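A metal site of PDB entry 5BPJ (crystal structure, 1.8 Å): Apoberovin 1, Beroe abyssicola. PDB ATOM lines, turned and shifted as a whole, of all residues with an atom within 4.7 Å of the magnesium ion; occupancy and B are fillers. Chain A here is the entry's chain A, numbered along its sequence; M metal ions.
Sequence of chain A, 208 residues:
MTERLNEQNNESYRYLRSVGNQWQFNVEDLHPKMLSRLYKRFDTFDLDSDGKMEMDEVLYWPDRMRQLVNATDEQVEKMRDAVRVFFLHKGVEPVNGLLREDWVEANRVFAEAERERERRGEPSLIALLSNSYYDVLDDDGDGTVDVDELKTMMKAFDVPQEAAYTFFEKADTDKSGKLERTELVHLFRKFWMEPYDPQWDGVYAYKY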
ATOM      1  N   ASP A  46      32.759 -17.198   1.636  1.00  0.00           N
ATOM      2  CA  ASP A  46      32.144 -18.073   0.630  1.00  0.00           C
ATOM      3  C   ASP A  46      33.374 -18.728   0.117  1.00  0.00           C
ATOM      4  O   ASP A  46      34.158 -18.135  -0.597  1.00  0.00           O
ATOM      5  CB  ASP A  46      31.488 -17.364  -0.560  1.00  0.00           C
ATOM      6  CG  ASP A  46      30.497 -18.227  -1.285  1.00  0.00           C
ATOM      7  OD1 ASP A  46      30.214 -19.391  -0.954  1.00  0.00           O
ATOM      8  OD2 ASP A  46      29.952 -17.670  -2.199  1.00  0.00           O
ATOM      9  N   LEU A  47      33.582 -19.917   0.607  1.00  0.00           N
ATOM     10  CA  LEU A  47      34.753 -20.645   0.228  1.00  0.00           C
ATOM     11  C   LEU A  47      34.596 -21.061  -1.212  1.00  0.00           C
ATOM     12  O   LEU A  47      35.490 -20.834  -1.980  1.00  0.00           O
ATOM     13  CB  LEU A  47      35.071 -21.818   1.179  1.00  0.00           C
ATOM     14  CG  LEU A  47      35.479 -21.434   2.619  1.00  0.00           C
ATOM     15  CD1 LEU A  47      35.580 -22.574   3.583  1.00  0.00           C
ATOM     16  CD2 LEU A  47      36.655 -20.519   2.680  1.00  0.00           C
ATOM     17  N   ASP A  48      33.440 -21.563  -1.591  1.00  0.00           N
ATOM     18  CA  ASP A  48      33.275 -21.980  -2.953  1.00  0.00           C
ATOM     19  C   ASP A  48      32.865 -20.880  -3.907  1.00  0.00           C
ATOM     20  O   ASP A  48      32.692 -21.127  -5.029  1.00  0.00           O
ATOM     21  CB  ASP A  48      32.378 -23.233  -3.104  1.00  0.00           C
ATOM     22  CG  ASP A  48      30.929 -22.958  -2.842  1.00  0.00           C
ATOM     23  OD1 ASP A  48      30.600 -21.803  -2.751  1.00  0.00           O
ATOM     24  OD2 ASP A  48      30.115 -23.901  -2.728  1.00  0.00           O
ATOM     25  N   SER A  49      32.737 -19.672  -3.437  1.00  0.00           N
ATOM     26  CA  SER A  49      32.440 -18.575  -4.292  1.00  0.00           C
ATOM     27  C   SER A  49      31.131 -18.711  -5.001  1.00  0.00           C
ATOM     28  O   SER A  49      30.919 -18.129  -6.006  1.00  0.00           O
ATOM     29  CB  SER A  49      33.544 -18.411  -5.282  1.00  0.00           C
ATOM     30  OG  SER A  49      34.643 -17.801  -4.714  1.00  0.00           O
ATOM     31  N   ASP A  50      30.240 -19.475  -4.445  1.00  0.00           N
ATOM     32  CA  ASP A  50      28.904 -19.589  -4.966  1.00  0.00           C
ATOM     33  C   ASP A  50      27.961 -18.478  -4.505  1.00  0.00           C
ATOM     34  O   ASP A  50      26.779 -18.553  -4.743  1.00  0.00           O
ATOM     35  CB  ASP A  50      28.319 -20.935  -4.576  1.00  0.00           C
ATOM     36  CG  ASP A  50      27.898 -20.983  -3.157  1.00  0.00           C
ATOM     37  OD1 ASP A  50      28.400 -20.204  -2.380  1.00  0.00           O
ATOM     38  OD2 ASP A  50      27.083 -21.817  -2.829  1.00  0.00           O
ATOM     39  N   LYS A  52      26.769 -17.848  -1.755  1.00  0.00           N
ATOM     40  CA  LYS A  52      26.005 -18.176  -0.555  1.00  0.00           C
ATOM     41  C   LYS A  52      26.960 -18.666   0.523  1.00  0.00           C
ATOM     42  O   LYS A  52      27.859 -19.456   0.245  1.00  0.00           O
ATOM     43  CB  LYS A  52      24.941 -19.235  -0.839  1.00  0.00           C
ATOM     44  CG  LYS A  52      23.832 -19.226   0.210  1.00  0.00           C
ATOM     45  CD  LYS A  52      23.289 -20.613   0.466  1.00  0.00           C
ATOM     46  CE  LYS A  52      22.699 -21.203  -0.782  1.00  0.00           C
ATOM     47  NZ  LYS A  52      22.465 -22.667  -0.611  1.00  0.00           N
ATOM     48  N   MET A  53      26.823 -18.195   1.768  1.00  0.00           N
ATOM     49  CA  MET A  53      27.600 -18.683   2.867  1.00  0.00           C
ATOM     50  C   MET A  53      26.805 -19.779   3.553  1.00  0.00           C
ATOM     51  O   MET A  53      25.653 -19.618   3.816  1.00  0.00           O
ATOM     52  CB  MET A  53      27.906 -17.567   3.841  1.00  0.00           C
ATOM     53  CG  MET A  53      29.130 -16.718   3.591  1.00  0.00           C
ATOM     54  SD  MET A  53      29.490 -15.408   4.763  1.00  0.00           S
ATOM     55  CE  MET A  53      29.335 -16.367   6.222  1.00  0.00           C
ATOM     56  N   GLU A  54      27.430 -20.910   3.842  1.00  0.00           N
ATOM     57  CA  GLU A  54      26.706 -22.043   4.395  1.00  0.00           C
ATOM     58  C   GLU A  54      27.340 -22.559   5.655  1.00  0.00           C
ATOM     59  O   GLU A  54      28.485 -22.395   5.856  1.00  0.00           O
ATOM     60  CB  GLU A  54      26.634 -23.217   3.422  1.00  0.00           C
ATOM     61  CG  GLU A  54      25.947 -23.009   2.100  1.00  0.00           C
ATOM     62  CD  GLU A  54      25.834 -24.291   1.280  1.00  0.00           C
ATOM     63  OE1 GLU A  54      26.725 -24.498   0.461  1.00  0.00           O
ATOM     64  OE2 GLU A  54      24.882 -25.085   1.477  1.00  0.00           O
ATOM     65  N   GLU A  57      30.339 -24.589   5.322  1.00  0.00           N
ATOM     66  CA  GLU A  57      31.455 -23.709   4.981  1.00  0.00           C
ATOM     67  C   GLU A  57      32.063 -23.003   6.172  1.00  0.00           C
ATOM     68  O   GLU A  57      33.275 -22.995   6.322  1.00  0.00           O
ATOM     69  CB  GLU A  57      31.031 -22.666   3.965  1.00  0.00           C
ATOM     70  CG  GLU A  57      31.208 -23.079   2.547  1.00  0.00           C
ATOM     71  CD  GLU A  57      30.730 -22.003   1.623  1.00  0.00           C
ATOM     72  OE1 GLU A  57      29.780 -21.288   2.013  1.00  0.00           O
ATOM     73  OE2 GLU A  57      31.317 -21.846   0.542  1.00  0.00           O
HETATM   74 MG    MG M   1      29.408 -20.863  -0.596  1.00  0.00          MG
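The backbone NH (N) of Asp 50 sits close to the side-chain carboxylate (OD1) of Asp 48 (2.9 Å). OE2 of Glu 57 lies close to N of Asp 48. The side-chain carboxylate (OE2) of Glu 57 sits close to the backbone NH (N) of Leu 47, 3.0 Å away. The backbone NH of Glu 54 lies within hydrogen-bond range of the side-chain carboxylate of Glu 57 (3.0 Å).
The magnesium ion is bound by OD1 of Asp 46, OD1 of Asp 50, O of Lys 52 and OE2 of Glu 57. Slightly farther from the magnesium ion lies the side-chain carboxylate (OD1) of Asp 48 (2.6 Å). Slightly farther from the magnesium ion lies OE1 of Glu 57 (2.7 Å).
The nearest printed residue that does not touch the magnesium ion is Met 53 (4.4 Å).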
